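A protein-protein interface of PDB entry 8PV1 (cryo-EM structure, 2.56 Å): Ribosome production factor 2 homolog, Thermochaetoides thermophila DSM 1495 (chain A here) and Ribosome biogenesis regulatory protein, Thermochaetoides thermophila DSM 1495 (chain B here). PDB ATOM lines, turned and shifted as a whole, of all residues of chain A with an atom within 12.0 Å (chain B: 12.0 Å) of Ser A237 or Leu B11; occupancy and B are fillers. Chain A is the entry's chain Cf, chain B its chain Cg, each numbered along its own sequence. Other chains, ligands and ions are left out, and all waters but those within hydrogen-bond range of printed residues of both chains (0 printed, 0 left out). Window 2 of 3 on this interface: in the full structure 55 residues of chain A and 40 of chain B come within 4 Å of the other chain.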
ATOM      1  N   ARG A 233       5.232  34.619   6.867  1.00  0.00           N
ATOM      2  CA  ARG A 233       4.441  34.925   5.688  1.00  0.00           C
ATOM      3  C   ARG A 233       4.771  33.924   4.588  1.00  0.00           C
ATOM      4  O   ARG A 233       5.904  33.447   4.483  1.00  0.00           O
ATOM      5  CB  ARG A 233       4.714  36.346   5.203  1.00  0.00           C
ATOM      6  CG  ARG A 233       4.214  37.431   6.137  1.00  0.00           C
ATOM      7  CD  ARG A 233       4.472  38.796   5.537  1.00  0.00           C
ATOM      8  NE  ARG A 233       5.901  39.083   5.510  1.00  0.00           N
ATOM      9  CZ  ARG A 233       6.626  39.193   4.405  1.00  0.00           C
ATOM     10  NH1 ARG A 233       6.085  39.049   3.206  1.00  0.00           N
ATOM     11  NH2 ARG A 233       7.928  39.446   4.506  1.00  0.00           N
ATOM     12  N   THR A 234       3.773  33.611   3.768  1.00  0.00           N
ATOM     13  CA  THR A 234       3.910  32.634   2.698  1.00  0.00           C
ATOM     14  C   THR A 234       3.663  33.300   1.353  1.00  0.00           C
ATOM     15  O   THR A 234       2.820  34.193   1.239  1.00  0.00           O
ATOM     16  CB  THR A 234       2.937  31.467   2.885  1.00  0.00           C
ATOM     17  OG1 THR A 234       1.602  31.973   3.014  1.00  0.00           O
ATOM     18  CG2 THR A 234       3.294  30.670   4.128  1.00  0.00           C
ATOM     19  N   LYS A 235       4.407  32.866   0.336  1.00  0.00           N
ATOM     20  CA  LYS A 235       4.327  33.434  -1.002  1.00  0.00           C
ATOM     21  C   LYS A 235       4.315  32.319  -2.041  1.00  0.00           C
ATOM     22  O   LYS A 235       4.736  31.191  -1.774  1.00  0.00           O
ATOM     23  CB  LYS A 235       5.497  34.387  -1.284  1.00  0.00           C
ATOM     24  CG  LYS A 235       5.490  35.661  -0.457  1.00  0.00           C
ATOM     25  CD  LYS A 235       6.640  36.571  -0.847  1.00  0.00           C
ATOM     26  CE  LYS A 235       6.697  37.801   0.044  1.00  0.00           C
ATOM     27  NZ  LYS A 235       5.525  38.694  -0.166  1.00  0.00           N
ATOM     28  N   ARG A 236       3.817  32.649  -3.232  1.00  0.00           N
ATOM     29  CA  ARG A 236       3.863  31.714  -4.350  1.00  0.00           C
ATOM     30  C   ARG A 236       5.295  31.540  -4.838  1.00  0.00           C
ATOM     31  O   ARG A 236       6.077  32.495  -4.862  1.00  0.00           O
ATOM     32  CB  ARG A 236       2.975  32.191  -5.500  1.00  0.00           C
ATOM     33  CG  ARG A 236       1.519  32.344  -5.130  1.00  0.00           C
ATOM     34  CD  ARG A 236       0.641  32.683  -6.315  1.00  0.00           C
ATOM     35  NE  ARG A 236      -0.760  32.755  -5.920  1.00  0.00           N
ATOM     36  CZ  ARG A 236      -1.575  31.711  -5.856  1.00  0.00           C
ATOM     37  NH1 ARG A 236      -1.163  30.492  -6.167  1.00  0.00           N
ATOM     38  NH2 ARG A 236      -2.834  31.892  -5.470  1.00  0.00           N
ATOM     39  N   SER A 237       5.636  30.313  -5.229  1.00  0.00           N
ATOM     40  CA  SER A 237       6.958  30.004  -5.756  1.00  0.00           C
ATOM     41  C   SER A 237       6.896  29.217  -7.059  1.00  0.00           C
ATOM     42  O   SER A 237       7.944  28.817  -7.580  1.00  0.00           O
ATOM     43  CB  SER A 237       7.772  29.233  -4.717  1.00  0.00           C
ATOM     44  OG  SER A 237       7.242  27.935  -4.521  1.00  0.00           O
ATOM     45  N   GLY A 238       5.702  28.985  -7.598  1.00  0.00           N
ATOM     46  CA  GLY A 238       5.545  28.192  -8.797  1.00  0.00           C
ATOM     47  C   GLY A 238       5.538  26.697  -8.579  1.00  0.00           C
ATOM     48  O   GLY A 238       5.363  25.949  -9.548  1.00  0.00           O
ATOM     49  N   THR A 239       5.722  26.236  -7.345  1.00  0.00           N
ATOM     50  CA  THR A 239       5.687  24.823  -6.997  1.00  0.00           C
ATOM     51  C   THR A 239       4.542  24.589  -6.019  1.00  0.00           C
ATOM     52  O   THR A 239       3.754  25.491  -5.724  1.00  0.00           O
ATOM     53  CB  THR A 239       7.020  24.358  -6.393  1.00  0.00           C
ATOM     54  OG1 THR A 239       7.111  24.801  -5.034  1.00  0.00           O
ATOM     55  CG2 THR A 239       8.198  24.913  -7.183  1.00  0.00           C
ATOM     56  N   ARG A 240       4.445  23.356  -5.519  1.00  0.00           N
ATOM     57  CA  ARG A 240       3.409  23.033  -4.543  1.00  0.00           C
ATOM     58  C   ARG A 240       3.712  23.660  -3.188  1.00  0.00           C
ATOM     59  O   ARG A 240       2.817  24.195  -2.524  1.00  0.00           O
ATOM     60  CB  ARG A 240       3.261  21.517  -4.419  1.00  0.00           C
ATOM     61  CG  ARG A 240       2.830  20.839  -5.705  1.00  0.00           C
ATOM     62  CD  ARG A 240       1.420  21.262  -6.080  1.00  0.00           C
ATOM     63  NE  ARG A 240       0.443  20.822  -5.090  1.00  0.00           N
ATOM     64  CZ  ARG A 240      -0.787  21.306  -4.982  1.00  0.00           C
ATOM     65  NH1 ARG A 240      -1.227  22.264  -5.781  1.00  0.00           N
ATOM     66  NH2 ARG A 240      -1.596  20.816  -4.045  1.00  0.00           N
ATOM     67  N   LEU A 241       4.969  23.604  -2.762  1.00  0.00           N
ATOM     68  CA  LEU A 241       5.332  24.136  -1.459  1.00  0.00           C
ATOM     69  C   LEU A 241       5.398  25.661  -1.505  1.00  0.00           C
ATOM     70  O   LEU A 241       5.849  26.235  -2.500  1.00  0.00           O
ATOM     71  CB  LEU A 241       6.674  23.564  -1.007  1.00  0.00           C
ATOM     72  CG  LEU A 241       6.651  22.067  -0.699  1.00  0.00           C
ATOM     73  CD1 LEU A 241       8.045  21.558  -0.384  1.00  0.00           C
ATOM     74  CD2 LEU A 241       5.701  21.779   0.447  1.00  0.00           C
ATOM     75  N   PRO A 242       4.956  26.343  -0.453  1.00  0.00           N
ATOM     76  CA  PRO A 242       5.012  27.806  -0.438  1.00  0.00           C
ATOM     77  C   PRO A 242       6.400  28.318  -0.082  1.00  0.00           C
ATOM     78  O   PRO A 242       7.227  27.619   0.503  1.00  0.00           O
ATOM     79  CB  PRO A 242       3.999  28.180   0.647  1.00  0.00           C
ATOM     80  CG  PRO A 242       4.052  27.035   1.592  1.00  0.00           C
ATOM     81  CD  PRO A 242       4.299  25.806   0.753  1.00  0.00           C
ATOM     82  N   ARG A 243       6.636  29.575  -0.442  1.00  0.00           N
ATOM     83  CA  ARG A 243       7.879  30.255  -0.111  1.00  0.00           C
ATOM     84  C   ARG A 243       7.695  31.003   1.203  1.00  0.00           C
ATOM     85  O   ARG A 243       6.822  31.871   1.312  1.00  0.00           O
ATOM     86  CB  ARG A 243       8.289  31.211  -1.230  1.00  0.00           C
ATOM     87  CG  ARG A 243       9.347  32.219  -0.825  1.00  0.00           C
ATOM     88  CD  ARG A 243      10.714  31.574  -0.732  1.00  0.00           C
ATOM     89  NE  ARG A 243      11.738  32.529  -0.330  1.00  0.00           N
ATOM     90  CZ  ARG A 243      13.033  32.256  -0.267  1.00  0.00           C
ATOM     91  NH1 ARG A 243      13.502  31.058  -0.574  1.00  0.00           N
ATOM     92  NH2 ARG A 243      13.879  33.209   0.114  1.00  0.00           N
ATOM     93  N   VAL A 244       8.512  30.668   2.192  1.00  0.00           N
ATOM     94  CA  VAL A 244       8.359  31.219   3.533  1.00  0.00           C
ATOM     95  C   VAL A 244       9.242  32.449   3.683  1.00  0.00           C
ATOM     96  O   VAL A 244      10.435  32.422   3.363  1.00  0.00           O
ATOM     97  CB  VAL A 244       8.700  30.152   4.588  1.00  0.00           C
ATOM     98  CG1 VAL A 244       8.606  30.732   5.986  1.00  0.00           C
ATOM     99  CG2 VAL A 244       7.779  28.954   4.442  1.00  0.00           C
ATOM    100  N   GLU A 245       8.648  33.541   4.161  1.00  0.00           N
ATOM    101  CA  GLU A 245       9.382  34.743   4.523  1.00  0.00           C
ATOM    102  C   GLU A 245       9.011  35.126   5.946  1.00  0.00           C
ATOM    103  O   GLU A 245       7.866  34.954   6.369  1.00  0.00           O
ATOM    104  CB  GLU A 245       9.087  35.906   3.564  1.00  0.00           C
ATOM    105  CG  GLU A 245       9.417  35.617   2.107  1.00  0.00           C
ATOM    106  CD  GLU A 245      10.911  35.579   1.832  1.00  0.00           C
ATOM    107  OE1 GLU A 245      11.685  36.141   2.635  1.00  0.00           O
ATOM    108  OE2 GLU A 245      11.312  34.984   0.809  1.00  0.00           O
ATOM    109  N   VAL A 246       9.987  35.650   6.684  1.00  0.00           N
ATOM    110  CA  VAL A 246       9.812  35.932   8.101  1.00  0.00           C
ATOM    111  C   VAL A 246       9.834  37.436   8.332  1.00  0.00           C
ATOM    112  O   VAL A 246      10.356  38.214   7.530  1.00  0.00           O
ATOM    113  CB  VAL A 246      10.880  35.240   8.971  1.00  0.00           C
ATOM    114  CG1 VAL A 246      10.704  33.734   8.930  1.00  0.00           C
ATOM    115  CG2 VAL A 246      12.272  35.635   8.516  1.00  0.00           C
ATOM    116  N   LEU B  11      11.927  31.960  -6.493  1.00  0.00           N
ATOM    117  CA  LEU B  11      12.720  31.713  -5.292  1.00  0.00           C
ATOM    118  C   LEU B  11      12.569  30.264  -4.840  1.00  0.00           C
ATOM    119  O   LEU B  11      11.468  29.715  -4.870  1.00  0.00           O
ATOM    120  CB  LEU B  11      12.318  32.668  -4.159  1.00  0.00           C
ATOM    121  CG  LEU B  11      12.904  34.088  -4.097  1.00  0.00           C
ATOM    122  CD1 LEU B  11      14.414  34.035  -3.889  1.00  0.00           C
ATOM    123  CD2 LEU B  11      12.546  34.961  -5.299  1.00  0.00           C
ATOM    124  N   PRO B  12      13.675  29.643  -4.434  1.00  0.00           N
ATOM    125  CA  PRO B  12      13.619  28.238  -4.017  1.00  0.00           C
ATOM    126  C   PRO B  12      12.905  28.064  -2.686  1.00  0.00           C
ATOM    127  O   PRO B  12      12.905  28.951  -1.828  1.00  0.00           O
ATOM    128  CB  PRO B  12      15.096  27.847  -3.907  1.00  0.00           C
ATOM    129  CG  PRO B  12      15.782  29.127  -3.576  1.00  0.00           C
ATOM    130  CD  PRO B  12      15.042  30.187  -4.348  1.00  0.00           C
ATOM    131  N   VAL B  13      12.293  26.895  -2.523  1.00  0.00           N
ATOM    132  CA  VAL B  13      11.638  26.517  -1.280  1.00  0.00           C
ATOM    133  C   VAL B  13      12.415  25.414  -0.566  1.00  0.00           C
ATOM    134  O   VAL B  13      11.913  24.813   0.381  1.00  0.00           O
ATOM    135  CB  VAL B  13      10.179  26.102  -1.520  1.00  0.00           C
ATOM    136  CG1 VAL B  13       9.375  27.282  -2.022  1.00  0.00           C
ATOM    137  CG2 VAL B  13      10.114  24.949  -2.503  1.00  0.00           C
ATOM    138  N   THR B  14      13.634  25.135  -1.017  1.00  0.00           N
ATOM    139  CA  THR B  14      14.492  24.136  -0.404  1.00  0.00           C
ATOM    140  C   THR B  14      15.875  24.732  -0.197  1.00  0.00           C
ATOM    141  O   THR B  14      16.405  25.421  -1.072  1.00  0.00           O
ATOM    142  CB  THR B  14      14.590  22.871  -1.270  1.00  0.00           C
ATOM    143  OG1 THR B  14      13.285  22.510  -1.740  1.00  0.00           O
ATOM    144  CG2 THR B  14      15.165  21.713  -0.469  1.00  0.00           C
ATOM    145  N   VAL B  15      16.456  24.468   0.968  1.00  0.00           N
ATOM    146  CA  VAL B  15      17.791  24.945   1.301  1.00  0.00           C
ATOM    147  C   VAL B  15      18.716  23.745   1.442  1.00  0.00           C
ATOM    148  O   VAL B  15      18.277  22.645   1.797  1.00  0.00           O
ATOM    149  CB  VAL B  15      17.796  25.809   2.581  1.00  0.00           C
ATOM    150  CG1 VAL B  15      16.917  27.033   2.389  1.00  0.00           C
ATOM    151  CG2 VAL B  15      17.332  25.010   3.784  1.00  0.00           C
ATOM    152  N   GLU B  16      19.991  23.954   1.128  1.00  0.00           N
ATOM    153  CA  GLU B  16      21.004  22.910   1.191  1.00  0.00           C
ATOM    154  C   GLU B  16      22.024  23.276   2.257  1.00  0.00           C
ATOM    155  O   GLU B  16      22.575  24.381   2.242  1.00  0.00           O
ATOM    156  CB  GLU B  16      21.690  22.725  -0.165  1.00  0.00           C
ATOM    157  CG  GLU B  16      22.705  21.594  -0.201  1.00  0.00           C
ATOM    158  CD  GLU B  16      22.066  20.226  -0.058  1.00  0.00           C
ATOM    159  OE1 GLU B  16      20.906  20.059  -0.489  1.00  0.00           O
ATOM    160  OE2 GLU B  16      22.725  19.316   0.487  1.00  0.00           O
ATOM    161  N   GLN B  49      19.870  40.527  10.164  1.00  0.00           N
ATOM    162  CA  GLN B  49      19.631  39.965   8.838  1.00  0.00           C
ATOM    163  C   GLN B  49      20.122  38.521   8.771  1.00  0.00           C
ATOM    164  O   GLN B  49      19.435  37.649   8.226  1.00  0.00           O
ATOM    165  CB  GLN B  49      20.297  40.857   7.780  1.00  0.00           C
ATOM    166  CG  GLN B  49      19.992  40.588   6.282  1.00  0.00           C
ATOM    167  CD  GLN B  49      20.535  39.282   5.722  1.00  0.00           C
ATOM    168  OE1 GLN B  49      21.606  38.819   6.117  1.00  0.00           O
ATOM    169  NE2 GLN B  49      19.794  38.681   4.799  1.00  0.00           N
ATOM    170  N   SER B  53      17.835  35.233   8.386  1.00  0.00           N
ATOM    171  CA  SER B  53      18.088  34.224   7.360  1.00  0.00           C
ATOM    172  C   SER B  53      18.079  32.819   7.952  1.00  0.00           C
ATOM    173  O   SER B  53      17.507  31.893   7.359  1.00  0.00           O
ATOM    174  CB  SER B  53      19.420  34.505   6.666  1.00  0.00           C
ATOM    175  OG  SER B  53      19.725  33.490   5.725  1.00  0.00           O
ATOM    176  N   ARG B  56      14.451  32.026   8.721  1.00  0.00           N
ATOM    177  CA  ARG B  56      13.719  31.736   7.495  1.00  0.00           C
ATOM    178  C   ARG B  56      14.031  30.340   6.981  1.00  0.00           C
ATOM    179  O   ARG B  56      13.130  29.628   6.524  1.00  0.00           O
ATOM    180  CB  ARG B  56      14.050  32.778   6.429  1.00  0.00           C
ATOM    181  CG  ARG B  56      12.962  32.973   5.395  1.00  0.00           C
ATOM    182  CD  ARG B  56      13.557  33.175   4.012  1.00  0.00           C
ATOM    183  NE  ARG B  56      14.408  32.059   3.616  1.00  0.00           N
ATOM    184  CZ  ARG B  56      13.965  30.923   3.096  1.00  0.00           C
ATOM    185  NH1 ARG B  56      12.677  30.718   2.880  1.00  0.00           N
ATOM    186  NH2 ARG B  56      14.838  29.970   2.784  1.00  0.00           N
ATOM    187  N   ASP B  57      15.303  29.931   7.050  1.00  0.00           N
ATOM    188  CA  ASP B  57      15.674  28.583   6.628  1.00  0.00           C
ATOM    189  C   ASP B  57      14.992  27.528   7.490  1.00  0.00           C
ATOM    190  O   ASP B  57      14.436  26.546   6.973  1.00  0.00           O
ATOM    191  CB  ASP B  57      17.193  28.421   6.688  1.00  0.00           C
ATOM    192  CG  ASP B  57      17.909  29.251   5.644  1.00  0.00           C
ATOM    193  OD1 ASP B  57      17.319  29.498   4.571  1.00  0.00           O
ATOM    194  OD2 ASP B  57      19.063  29.656   5.896  1.00  0.00           O
ATOM    195  N   GLN B  60      11.258  27.446   6.769  1.00  0.00           N
ATOM    196  CA  GLN B  60      11.004  26.847   5.464  1.00  0.00           C
ATOM    197  C   GLN B  60      11.080  25.328   5.525  1.00  0.00           C
ATOM    198  O   GLN B  60      10.190  24.635   5.013  1.00  0.00           O
ATOM    199  CB  GLN B  60      11.995  27.393   4.437  1.00  0.00           C
ATOM    200  CG  GLN B  60      11.818  26.815   3.046  1.00  0.00           C
ATOM    201  CD  GLN B  60      10.623  27.395   2.321  1.00  0.00           C
ATOM    202  OE1 GLN B  60      10.570  28.594   2.050  1.00  0.00           O
ATOM    203  NE2 GLN B  60       9.649  26.548   2.012  1.00  0.00           N
ATOM    204  N   ILE B  63       8.046  23.984   7.517  1.00  0.00           N
ATOM    205  CA  ILE B  63       6.811  24.023   6.737  1.00  0.00           C
ATOM    206  C   ILE B  63       6.813  22.927   5.678  1.00  0.00           C
ATOM    207  O   ILE B  63       5.796  22.255   5.461  1.00  0.00           O
ATOM    208  CB  ILE B  63       6.616  25.424   6.123  1.00  0.00           C
ATOM    209  CG1 ILE B  63       6.217  26.431   7.205  1.00  0.00           C
ATOM    210  CG2 ILE B  63       5.569  25.412   5.019  1.00  0.00           C
ATOM    211  CD1 ILE B  63       4.966  26.056   7.960  1.00  0.00           C
ATOM    212  N   ASN B  64       7.960  22.714   5.021  1.00  0.00           N
ATOM    213  CA  ASN B  64       8.060  21.648   4.027  1.00  0.00           C
ATOM    214  C   ASN B  64       7.857  20.274   4.655  1.00  0.00           C
ATOM    215  O   ASN B  64       7.149  19.427   4.096  1.00  0.00           O
ATOM    216  CB  ASN B  64       9.413  21.712   3.322  1.00  0.00           C
ATOM    217  CG  ASN B  64       9.583  22.971   2.501  1.00  0.00           C
ATOM    218  OD1 ASN B  64       8.611  23.649   2.174  1.00  0.00           O
ATOM    219  ND2 ASN B  64      10.825  23.292   2.163  1.00  0.00           N
ATOM    220  N   LEU B  67       4.127  19.877   5.559  1.00  0.00           N
ATOM    221  CA  LEU B  67       3.248  19.747   4.406  1.00  0.00           C
ATOM    222  C   LEU B  67       3.537  18.514   3.561  1.00  0.00           C
ATOM    223  O   LEU B  67       2.690  18.142   2.743  1.00  0.00           O
ATOM    224  CB  LEU B  67       3.339  20.997   3.531  1.00  0.00           C
ATOM    225  CG  LEU B  67       2.701  22.259   4.117  1.00  0.00           C
ATOM    226  CD1 LEU B  67       2.739  23.393   3.113  1.00  0.00           C
ATOM    227  CD2 LEU B  67       1.280  21.988   4.567  1.00  0.00           C
ATOM    228  N   THR B  68       4.693  17.868   3.728  1.00  0.00           N
ATOM    229  CA  THR B  68       4.997  16.682   2.942  1.00  0.00           C
ATOM    230  C   THR B  68       4.862  15.364   3.689  1.00  0.00           C
ATOM    231  O   THR B  68       4.384  14.395   3.090  1.00  0.00           O
ATOM    232  CB  THR B  68       6.417  16.764   2.358  1.00  0.00           C
ATOM    233  OG1 THR B  68       7.358  17.016   3.409  1.00  0.00           O
ATOM    234  CG2 THR B  68       6.503  17.861   1.308  1.00  0.00           C
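Ser A237 touches Leu B11 (CB to O, 3.7 Å). Val B13 touches Ser A237. CD2 of Leu A241 touches CB of Leu B67 (3.96 Å). O of Pro A242 touches CG1 of Val B13, at 3.3 Å. CD of Pro A242 touches CD1 of Leu B67, 3.7 Å away. Arg A243 touches Val B13. Arg A243 touches Arg B56 (CZ to NH1, 3.5 Å). Arg A243 touches Gln B60. OE1 of Glu A245 touches CD of Arg B56 (3.8 Å). CG1 of Val A246 touches CA of Arg B56, at 3.9 Å.
Printed residues of chain B that touch a printed residue of chain A: Leu B11, Pro B12, Val B13, Arg B56, Gln B60, Asn B64 and Leu B67. Of the 14 printed residues of chain A, 8 touch a printed residue of chain B. Printed residues of chain A that touch a printed residue of chain B: Ser A237, Thr A239, Leu A241, Pro A242, Arg A243, Val A244, Glu A245 and Val A246. Hydrophobic or aromatic side chains of chain A within 4 Å of the printed part of chain B: Leu A241, Pro A242, Val A244 and Val A246. Among the printed residues, 18 pairs touch across the chains.
The side-chain amide nitrogen of Gln B60 is in hydrogen-bond range of the backbone carbonyl oxygen of Pro A242. The backbone carbonyl oxygen (O) of Pro B12 is in hydrogen-bond range of the guanidinium group (NH1) of Arg A243, 2.5 Å away. O of Val A244 is in hydrogen-bond range of NH1 of Arg B56 (2.9 Å). N of Val A244 sits at hydrogen-bond distance from OE1 of Gln B60, at 2.9 Å.
The backbone carbonyl oxygen of Arg A243 lies within hydrogen-bond range of the backbone NH of Lys A235, 2.8 Å away. OG of Ser A237 is in hydrogen-bond range of OG1 of Thr A239, at 3.2 Å. OG1 of Thr A239 sits at hydrogen-bond distance from O of Leu A241, at 3.2 Å. NE2 of Gln B60 lies within hydrogen-bond range of O of Val B13, 3.3 Å away. NE2 of Gln B60 sits at hydrogen-bond distance from OD1 of Asn B64 (3.1 Å). OG1 of Thr B68 sits at hydrogen-bond distance from O of Asn B64, at 2.5 Å.
Ser A237 touches just these residues of chain B: Leu B11 (3.7 Å) and Val B13 (3.3 Å). Leu B11 touches just these residues of chain A: Ser A237 (3.7 Å) and Arg A243 (3.9 Å). No residue of chain B comes within 4 Å of Gly A238. Of chain B, only Val B13 (3.9 Å) comes within 4 Å of Thr A239. Pro A242 touches three residues of chain B. Of chain B, only Leu B11, Pro B12, Val B13, Arg B56 and Gln B60 come within 4 Å of Arg A243. Of chain A, only Arg A243 (2.5 Å) comes within 4 Å of Pro B12. Printed residues of chain A within 4 Å of Arg B56: Arg A243, Val A244, Glu A245 and Val A246. Printed residues of chain A within 4 Å of Gln B60: Pro A242 (3.0 Å), Arg A243 (3.8 Å) and Val A244 (2.9 Å). Asp B57 touches none of the printed residues of chain A. The nearest residue of chain A that does not touch Leu B11 is Glu A245 (5.2 Å). The nearest printed residue of chain B that does not touch Leu A241 is Thr B68 (4.1 Å).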
